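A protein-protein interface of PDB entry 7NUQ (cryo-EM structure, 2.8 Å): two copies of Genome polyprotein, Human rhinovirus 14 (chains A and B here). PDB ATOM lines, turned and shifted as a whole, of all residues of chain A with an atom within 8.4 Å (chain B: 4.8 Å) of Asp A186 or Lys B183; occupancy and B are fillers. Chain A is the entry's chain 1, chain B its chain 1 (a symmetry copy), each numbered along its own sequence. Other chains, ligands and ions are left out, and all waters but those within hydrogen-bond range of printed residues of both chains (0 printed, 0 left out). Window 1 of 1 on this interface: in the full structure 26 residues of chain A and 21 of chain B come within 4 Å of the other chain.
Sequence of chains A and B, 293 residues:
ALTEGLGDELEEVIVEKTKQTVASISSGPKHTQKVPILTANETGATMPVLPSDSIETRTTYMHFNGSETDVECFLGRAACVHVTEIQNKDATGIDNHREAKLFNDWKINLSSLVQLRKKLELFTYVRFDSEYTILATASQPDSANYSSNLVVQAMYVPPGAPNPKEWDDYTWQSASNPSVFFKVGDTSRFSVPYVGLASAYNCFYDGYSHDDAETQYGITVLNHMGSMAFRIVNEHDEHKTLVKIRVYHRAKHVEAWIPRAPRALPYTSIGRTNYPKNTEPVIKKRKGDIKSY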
ATOM      1  N   THR A 133      28.544  -8.432  14.406  1.00  0.00           N
ATOM      2  CA  THR A 133      27.350  -7.696  14.009  1.00  0.00           C
ATOM      3  C   THR A 133      27.781  -6.594  13.056  1.00  0.00           C
ATOM      4  O   THR A 133      28.565  -5.717  13.434  1.00  0.00           O
ATOM      5  CB  THR A 133      26.626  -7.107  15.224  1.00  0.00           C
ATOM      6  OG1 THR A 133      26.588  -8.075  16.279  1.00  0.00           O
ATOM      7  CG2 THR A 133      25.205  -6.711  14.859  1.00  0.00           C
ATOM      8  N   ILE A 134      27.273  -6.635  11.827  1.00  0.00           N
ATOM      9  CA  ILE A 134      27.669  -5.706  10.774  1.00  0.00           C
ATOM     10  C   ILE A 134      26.558  -4.678  10.616  1.00  0.00           C
ATOM     11  O   ILE A 134      25.448  -5.015  10.185  1.00  0.00           O
ATOM     12  CB  ILE A 134      27.946  -6.431   9.448  1.00  0.00           C
ATOM     13  CG1 ILE A 134      28.745  -7.714   9.696  1.00  0.00           C
ATOM     14  CG2 ILE A 134      28.710  -5.518   8.506  1.00  0.00           C
ATOM     15  CD1 ILE A 134      29.124  -8.461   8.437  1.00  0.00           C
ATOM     16  N   LEU A 135      26.858  -3.424  10.952  1.00  0.00           N
ATOM     17  CA  LEU A 135      25.864  -2.355  10.999  1.00  0.00           C
ATOM     18  C   LEU A 135      26.053  -1.435   9.799  1.00  0.00           C
ATOM     19  O   LEU A 135      27.052  -0.714   9.713  1.00  0.00           O
ATOM     20  CB  LEU A 135      25.969  -1.579  12.312  1.00  0.00           C
ATOM     21  CG  LEU A 135      25.003  -0.412  12.525  1.00  0.00           C
ATOM     22  CD1 LEU A 135      23.630  -0.693  11.925  1.00  0.00           C
ATOM     23  CD2 LEU A 135      24.878  -0.121  14.010  1.00  0.00           C
ATOM     24  N   ALA A 136      25.090  -1.461   8.880  1.00  0.00           N
ATOM     25  CA  ALA A 136      25.081  -0.594   7.708  1.00  0.00           C
ATOM     26  C   ALA A 136      23.856   0.309   7.763  1.00  0.00           C
ATOM     27  O   ALA A 136      22.763  -0.143   8.114  1.00  0.00           O
ATOM     28  CB  ALA A 136      25.068  -1.419   6.421  1.00  0.00           C
ATOM     29  N   THR A 137      24.041   1.582   7.422  1.00  0.00           N
ATOM     30  CA  THR A 137      22.959   2.558   7.427  1.00  0.00           C
ATOM     31  C   THR A 137      22.910   3.256   6.075  1.00  0.00           C
ATOM     32  O   THR A 137      23.949   3.662   5.545  1.00  0.00           O
ATOM     33  CB  THR A 137      23.143   3.591   8.545  1.00  0.00           C
ATOM     34  OG1 THR A 137      24.305   4.387   8.280  1.00  0.00           O
ATOM     35  CG2 THR A 137      23.294   2.899   9.895  1.00  0.00           C
ATOM     36  N   ALA A 138      21.708   3.396   5.528  1.00  0.00           N
ATOM     37  CA  ALA A 138      21.502   4.061   4.252  1.00  0.00           C
ATOM     38  C   ALA A 138      21.363   5.565   4.459  1.00  0.00           C
ATOM     39  O   ALA A 138      20.826   6.032   5.468  1.00  0.00           O
ATOM     40  CB  ALA A 138      20.263   3.503   3.544  1.00  0.00           C
ATOM     41  N   LEU A 150      17.910  -1.896   0.471  1.00  0.00           N
ATOM     42  CA  LEU A 150      19.129  -2.607   0.117  1.00  0.00           C
ATOM     43  C   LEU A 150      19.128  -4.019   0.687  1.00  0.00           C
ATOM     44  O   LEU A 150      18.382  -4.342   1.616  1.00  0.00           O
ATOM     45  CB  LEU A 150      20.348  -1.837   0.626  1.00  0.00           C
ATOM     46  CG  LEU A 150      20.413  -0.382   0.148  1.00  0.00           C
ATOM     47  CD1 LEU A 150      21.498   0.379   0.888  1.00  0.00           C
ATOM     48  CD2 LEU A 150      20.634  -0.325  -1.359  1.00  0.00           C
ATOM     49  N   VAL A 152      22.356  -6.252   1.694  1.00  0.00           N
ATOM     50  CA  VAL A 152      23.809  -6.312   1.797  1.00  0.00           C
ATOM     51  C   VAL A 152      24.256  -7.761   1.910  1.00  0.00           C
ATOM     52  O   VAL A 152      23.713  -8.536   2.703  1.00  0.00           O
ATOM     53  CB  VAL A 152      24.303  -5.486   2.999  1.00  0.00           C
ATOM     54  CG1 VAL A 152      25.787  -5.725   3.244  1.00  0.00           C
ATOM     55  CG2 VAL A 152      24.030  -4.017   2.767  1.00  0.00           C
ATOM     56  N   VAL A 180      26.293 -13.932   4.071  1.00  0.00           N
ATOM     57  CA  VAL A 180      25.107 -13.574   4.837  1.00  0.00           C
ATOM     58  C   VAL A 180      24.414 -12.420   4.132  1.00  0.00           C
ATOM     59  O   VAL A 180      24.997 -11.344   3.961  1.00  0.00           O
ATOM     60  CB  VAL A 180      25.450 -13.190   6.290  1.00  0.00           C
ATOM     61  CG1 VAL A 180      24.197 -12.732   7.013  1.00  0.00           C
ATOM     62  CG2 VAL A 180      26.099 -14.362   7.016  1.00  0.00           C
ATOM     63  N   PHE A 181      23.167 -12.644   3.726  1.00  0.00           N
ATOM     64  CA  PHE A 181      22.366 -11.636   3.047  1.00  0.00           C
ATOM     65  C   PHE A 181      21.425 -10.984   4.048  1.00  0.00           C
ATOM     66  O   PHE A 181      20.859 -11.660   4.912  1.00  0.00           O
ATOM     67  CB  PHE A 181      21.584 -12.253   1.886  1.00  0.00           C
ATOM     68  CG  PHE A 181      22.461 -12.789   0.794  1.00  0.00           C
ATOM     69  CD1 PHE A 181      22.931 -14.089   0.843  1.00  0.00           C
ATOM     70  CD2 PHE A 181      22.828 -11.989  -0.274  1.00  0.00           C
ATOM     71  CE1 PHE A 181      23.740 -14.586  -0.155  1.00  0.00           C
ATOM     72  CE2 PHE A 181      23.641 -12.482  -1.277  1.00  0.00           C
ATOM     73  CZ  PHE A 181      24.096 -13.783  -1.216  1.00  0.00           C
ATOM     74  N   PHE A 182      21.277  -9.665   3.936  1.00  0.00           N
ATOM     75  CA  PHE A 182      20.477  -8.890   4.869  1.00  0.00           C
ATOM     76  C   PHE A 182      20.337  -7.476   4.327  1.00  0.00           C
ATOM     77  O   PHE A 182      21.139  -7.035   3.500  1.00  0.00           O
ATOM     78  CB  PHE A 182      21.106  -8.862   6.267  1.00  0.00           C
ATOM     79  CG  PHE A 182      22.505  -8.316   6.289  1.00  0.00           C
ATOM     80  CD1 PHE A 182      23.575  -9.101   5.896  1.00  0.00           C
ATOM     81  CD2 PHE A 182      22.750  -7.015   6.705  1.00  0.00           C
ATOM     82  CE1 PHE A 182      24.863  -8.601   5.916  1.00  0.00           C
ATOM     83  CE2 PHE A 182      24.037  -6.509   6.730  1.00  0.00           C
ATOM     84  CZ  PHE A 182      25.097  -7.304   6.334  1.00  0.00           C
ATOM     85  N   LYS A 183      19.313  -6.774   4.797  1.00  0.00           N
ATOM     86  CA  LYS A 183      19.067  -5.409   4.354  1.00  0.00           C
ATOM     87  C   LYS A 183      19.851  -4.418   5.208  1.00  0.00           C
ATOM     88  O   LYS A 183      20.216  -4.711   6.350  1.00  0.00           O
ATOM     89  CB  LYS A 183      17.571  -5.094   4.414  1.00  0.00           C
ATOM     90  CG  LYS A 183      16.702  -6.095   3.655  1.00  0.00           C
ATOM     91  CD  LYS A 183      15.238  -5.677   3.608  1.00  0.00           C
ATOM     92  CE  LYS A 183      14.590  -5.672   4.989  1.00  0.00           C
ATOM     93  NZ  LYS A 183      14.604  -7.008   5.641  1.00  0.00           N
ATOM     94  N   VAL A 184      20.111  -3.238   4.640  1.00  0.00           N
ATOM     95  CA  VAL A 184      20.851  -2.202   5.352  1.00  0.00           C
ATOM     96  C   VAL A 184      20.049  -1.738   6.560  1.00  0.00           C
ATOM     97  O   VAL A 184      18.816  -1.623   6.509  1.00  0.00           O
ATOM     98  CB  VAL A 184      21.172  -1.030   4.407  1.00  0.00           C
ATOM     99  CG1 VAL A 184      21.288   0.279   5.173  1.00  0.00           C
ATOM    100  CG2 VAL A 184      22.457  -1.300   3.641  1.00  0.00           C
ATOM    101  N   GLY A 185      20.752  -1.466   7.658  1.00  0.00           N
ATOM    102  CA  GLY A 185      20.111  -1.045   8.887  1.00  0.00           C
ATOM    103  C   GLY A 185      19.947  -2.196   9.857  1.00  0.00           C
ATOM    104  O   GLY A 185      20.151  -2.043  11.065  1.00  0.00           O
ATOM    105  N   ASP A 186      19.571  -3.354   9.330  1.00  0.00           N
ATOM    106  CA  ASP A 186      19.511  -4.583  10.100  1.00  0.00           C
ATOM    107  C   ASP A 186      20.838  -5.320   9.948  1.00  0.00           C
ATOM    108  O   ASP A 186      21.551  -5.168   8.950  1.00  0.00           O
ATOM    109  CB  ASP A 186      18.315  -5.424   9.651  1.00  0.00           C
ATOM    110  CG  ASP A 186      16.992  -4.824  10.081  1.00  0.00           C
ATOM    111  OD1 ASP A 186      16.880  -4.393  11.246  1.00  0.00           O
ATOM    112  OD2 ASP A 186      16.063  -4.779   9.247  1.00  0.00           O
ATOM    113  N   THR A 187      21.181  -6.132  10.945  1.00  0.00           N
ATOM    114  CA  THR A 187      22.527  -6.666  11.062  1.00  0.00           C
ATOM    115  C   THR A 187      22.492  -8.186  11.010  1.00  0.00           C
ATOM    116  O   THR A 187      21.485  -8.822  11.331  1.00  0.00           O
ATOM    117  CB  THR A 187      23.193  -6.206  12.365  1.00  0.00           C
ATOM    118  OG1 THR A 187      22.463  -6.722  13.486  1.00  0.00           O
ATOM    119  CG2 THR A 187      23.226  -4.680  12.446  1.00  0.00           C
ATOM    120  N   SER A 188      23.623  -8.759  10.610  1.00  0.00           N
ATOM    121  CA  SER A 188      23.815 -10.199  10.574  1.00  0.00           C
ATOM    122  C   SER A 188      24.387 -10.659  11.905  1.00  0.00           C
ATOM    123  O   SER A 188      25.008  -9.881  12.635  1.00  0.00           O
ATOM    124  CB  SER A 188      24.754 -10.605   9.432  1.00  0.00           C
ATOM    125  OG  SER A 188      25.970  -9.878   9.492  1.00  0.00           O
ATOM    126  N   ARG A 189      24.171 -11.935  12.217  1.00  0.00           N
ATOM    127  CA  ARG A 189      24.610 -12.490  13.493  1.00  0.00           C
ATOM    128  C   ARG A 189      25.070 -13.919  13.249  1.00  0.00           C
ATOM    129  O   ARG A 189      24.258 -14.848  13.284  1.00  0.00           O
ATOM    130  CB  ARG A 189      23.487 -12.434  14.526  1.00  0.00           C
ATOM    131  CG  ARG A 189      23.855 -12.963  15.903  1.00  0.00           C
ATOM    132  CD  ARG A 189      24.969 -12.162  16.550  1.00  0.00           C
ATOM    133  NE  ARG A 189      24.574 -10.783  16.838  1.00  0.00           N
ATOM    134  CZ  ARG A 189      24.038 -10.376  17.987  1.00  0.00           C
ATOM    135  NH1 ARG A 189      23.819 -11.235  18.975  1.00  0.00           N
ATOM    136  NH2 ARG A 189      23.715  -9.100  18.145  1.00  0.00           N
ATOM    137  N   LEU B 150      16.774   5.110   9.767  1.00  0.00           N
ATOM    138  CA  LEU B 150      17.814   5.401  10.741  1.00  0.00           C
ATOM    139  C   LEU B 150      18.131   4.178  11.591  1.00  0.00           C
ATOM    140  O   LEU B 150      17.347   3.228  11.675  1.00  0.00           O
ATOM    141  CB  LEU B 150      17.378   6.562  11.637  1.00  0.00           C
ATOM    142  CG  LEU B 150      16.986   7.829  10.870  1.00  0.00           C
ATOM    143  CD1 LEU B 150      16.332   8.839  11.798  1.00  0.00           C
ATOM    144  CD2 LEU B 150      18.200   8.431  10.175  1.00  0.00           C
ATOM    145  N   VAL B 151      19.312   4.203  12.204  1.00  0.00           N
ATOM    146  CA  VAL B 151      19.738   3.191  13.161  1.00  0.00           C
ATOM    147  C   VAL B 151      20.352   3.921  14.349  1.00  0.00           C
ATOM    148  O   VAL B 151      21.538   4.277  14.319  1.00  0.00           O
ATOM    149  CB  VAL B 151      20.739   2.201  12.542  1.00  0.00           C
ATOM    150  CG1 VAL B 151      20.972   1.025  13.475  1.00  0.00           C
ATOM    151  CG2 VAL B 151      20.235   1.722  11.190  1.00  0.00           C
ATOM    152  N   VAL B 152      19.554   4.136  15.385  1.00  0.00           N
ATOM    153  CA  VAL B 152      19.958   4.926  16.540  1.00  0.00           C
ATOM    154  C   VAL B 152      20.791   4.071  17.481  1.00  0.00           C
ATOM    155  O   VAL B 152      20.422   2.941  17.812  1.00  0.00           O
ATOM    156  CB  VAL B 152      18.724   5.501  17.262  1.00  0.00           C
ATOM    157  CG1 VAL B 152      19.124   6.135  18.588  1.00  0.00           C
ATOM    158  CG2 VAL B 152      18.027   6.509  16.377  1.00  0.00           C
ATOM    159  N   PHE B 181      21.673  -0.763  19.526  1.00  0.00           N
ATOM    160  CA  PHE B 181      21.410  -0.289  18.175  1.00  0.00           C
ATOM    161  C   PHE B 181      19.984  -0.643  17.787  1.00  0.00           C
ATOM    162  O   PHE B 181      19.497  -1.733  18.104  1.00  0.00           O
ATOM    163  CB  PHE B 181      22.408  -0.889  17.183  1.00  0.00           C
ATOM    164  CG  PHE B 181      23.824  -0.462  17.428  1.00  0.00           C
ATOM    165  CD1 PHE B 181      24.636  -1.173  18.295  1.00  0.00           C
ATOM    166  CD2 PHE B 181      24.341   0.661  16.805  1.00  0.00           C
ATOM    167  CE1 PHE B 181      25.936  -0.781  18.528  1.00  0.00           C
ATOM    168  CE2 PHE B 181      25.645   1.058  17.037  1.00  0.00           C
ATOM    169  CZ  PHE B 181      26.442   0.334  17.898  1.00  0.00           C
ATOM    170  N   PHE B 182      19.312   0.293  17.118  1.00  0.00           N
ATOM    171  CA  PHE B 182      17.914   0.134  16.751  1.00  0.00           C
ATOM    172  C   PHE B 182      17.530   1.267  15.813  1.00  0.00           C
ATOM    173  O   PHE B 182      18.188   2.311  15.781  1.00  0.00           O
ATOM    174  CB  PHE B 182      17.002   0.133  17.983  1.00  0.00           C
ATOM    175  CG  PHE B 182      17.125   1.371  18.826  1.00  0.00           C
ATOM    176  CD1 PHE B 182      18.189   1.529  19.696  1.00  0.00           C
ATOM    177  CD2 PHE B 182      16.172   2.376  18.748  1.00  0.00           C
ATOM    178  CE1 PHE B 182      18.302   2.666  20.473  1.00  0.00           C
ATOM    179  CE2 PHE B 182      16.279   3.516  19.524  1.00  0.00           C
ATOM    180  CZ  PHE B 182      17.347   3.662  20.389  1.00  0.00           C
ATOM    181  N   LYS B 183      16.465   1.052  15.050  1.00  0.00           N
ATOM    182  CA  LYS B 183      15.997   2.058  14.107  1.00  0.00           C
ATOM    183  C   LYS B 183      15.037   3.027  14.788  1.00  0.00           C
ATOM    184  O   LYS B 183      14.417   2.701  15.803  1.00  0.00           O
ATOM    185  CB  LYS B 183      15.316   1.387  12.913  1.00  0.00           C
ATOM    186  CG  LYS B 183      16.179   0.332  12.224  1.00  0.00           C
ATOM    187  CD  LYS B 183      15.535  -0.213  10.956  1.00  0.00           C
ATOM    188  CE  LYS B 183      14.252  -0.986  11.241  1.00  0.00           C
ATOM    189  NZ  LYS B 183      14.469  -2.167  12.119  1.00  0.00           N
ATOM    190  N   VAL B 184      14.924   4.230  14.219  1.00  0.00           N
ATOM    191  CA  VAL B 184      14.037   5.249  14.772  1.00  0.00           C
ATOM    192  C   VAL B 184      12.593   4.776  14.675  1.00  0.00           C
ATOM    193  O   VAL B 184      12.188   4.143  13.689  1.00  0.00           O
ATOM    194  CB  VAL B 184      14.242   6.588  14.043  1.00  0.00           C
ATOM    195  CG1 VAL B 184      12.972   7.425  14.061  1.00  0.00           C
ATOM    196  CG2 VAL B 184      15.386   7.367  14.672  1.00  0.00           C
ATOM    197  N   GLY B 185      11.805   5.089  15.702  1.00  0.00           N
ATOM    198  CA  GLY B 185      10.417   4.676  15.751  1.00  0.00           C
ATOM    199  C   GLY B 185      10.231   3.438  16.602  1.00  0.00           C
ATOM    200  O   GLY B 185       9.267   3.333  17.368  1.00  0.00           O
ATOM    201  N   ASP B 186      11.153   2.492  16.468  1.00  0.00           N
ATOM    202  CA  ASP B 186      11.196   1.315  17.316  1.00  0.00           C
ATOM    203  C   ASP B 186      12.126   1.594  18.493  1.00  0.00           C
ATOM    204  O   ASP B 186      13.046   2.415  18.409  1.00  0.00           O
ATOM    205  CB  ASP B 186      11.630   0.098  16.498  1.00  0.00           C
ATOM    206  CG  ASP B 186      10.559  -0.361  15.530  1.00  0.00           C
ATOM    207  OD1 ASP B 186       9.380  -0.434  15.931  1.00  0.00           O
ATOM    208  OD2 ASP B 186      10.898  -0.643  14.362  1.00  0.00           O
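NZ of Lys B183 is in salt-bridge range of OD1 of Asp A186 (3.4 Å).
The backbone carbonyl oxygen of Ala A136 is in hydrogen-bond range of the backbone NH of Gly A185, at 2.4 Å.
Among the printed residues, pairs that only touch across the chains: Leu A135 with Val B151, Leu A135 with Phe B181, Thr A137 with Val B151 and Gly A185 with Val B151.
Printed residues of chain B within 4 Å of Gly A185: Val B151. Asp A186 touches one residue of chain B. Printed residues of chain A within 4 Å of Val B151: Leu A135, Thr A137 and Gly A185. Lys B183 touches one residue of chain A. The nearest residue of chain A that does not touch Lys B183 is Gly A185 (4.8 Å).
Hydrophobic or aromatic side chains of chain A within 4 Å of the printed part of chain B: Leu A135. Printed residues of chain B that touch a printed residue of chain A: Val B151, Phe B181 and Lys B183. Hydrophobic or aromatic side chains of chain B that line the printed part of chain A: Val B151 and Phe B181. Along chain B the printed residues that touch a printed residue of chain A span positions 151 to 183.
Asp A186 touches Lys B183, but with the chains exchanged Lys A183 does not touch Asp B186 (11.3 Å). Of the 5 pairs that touch across the chains among the printed residues, none has its exchanged pair printed and touching as well.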
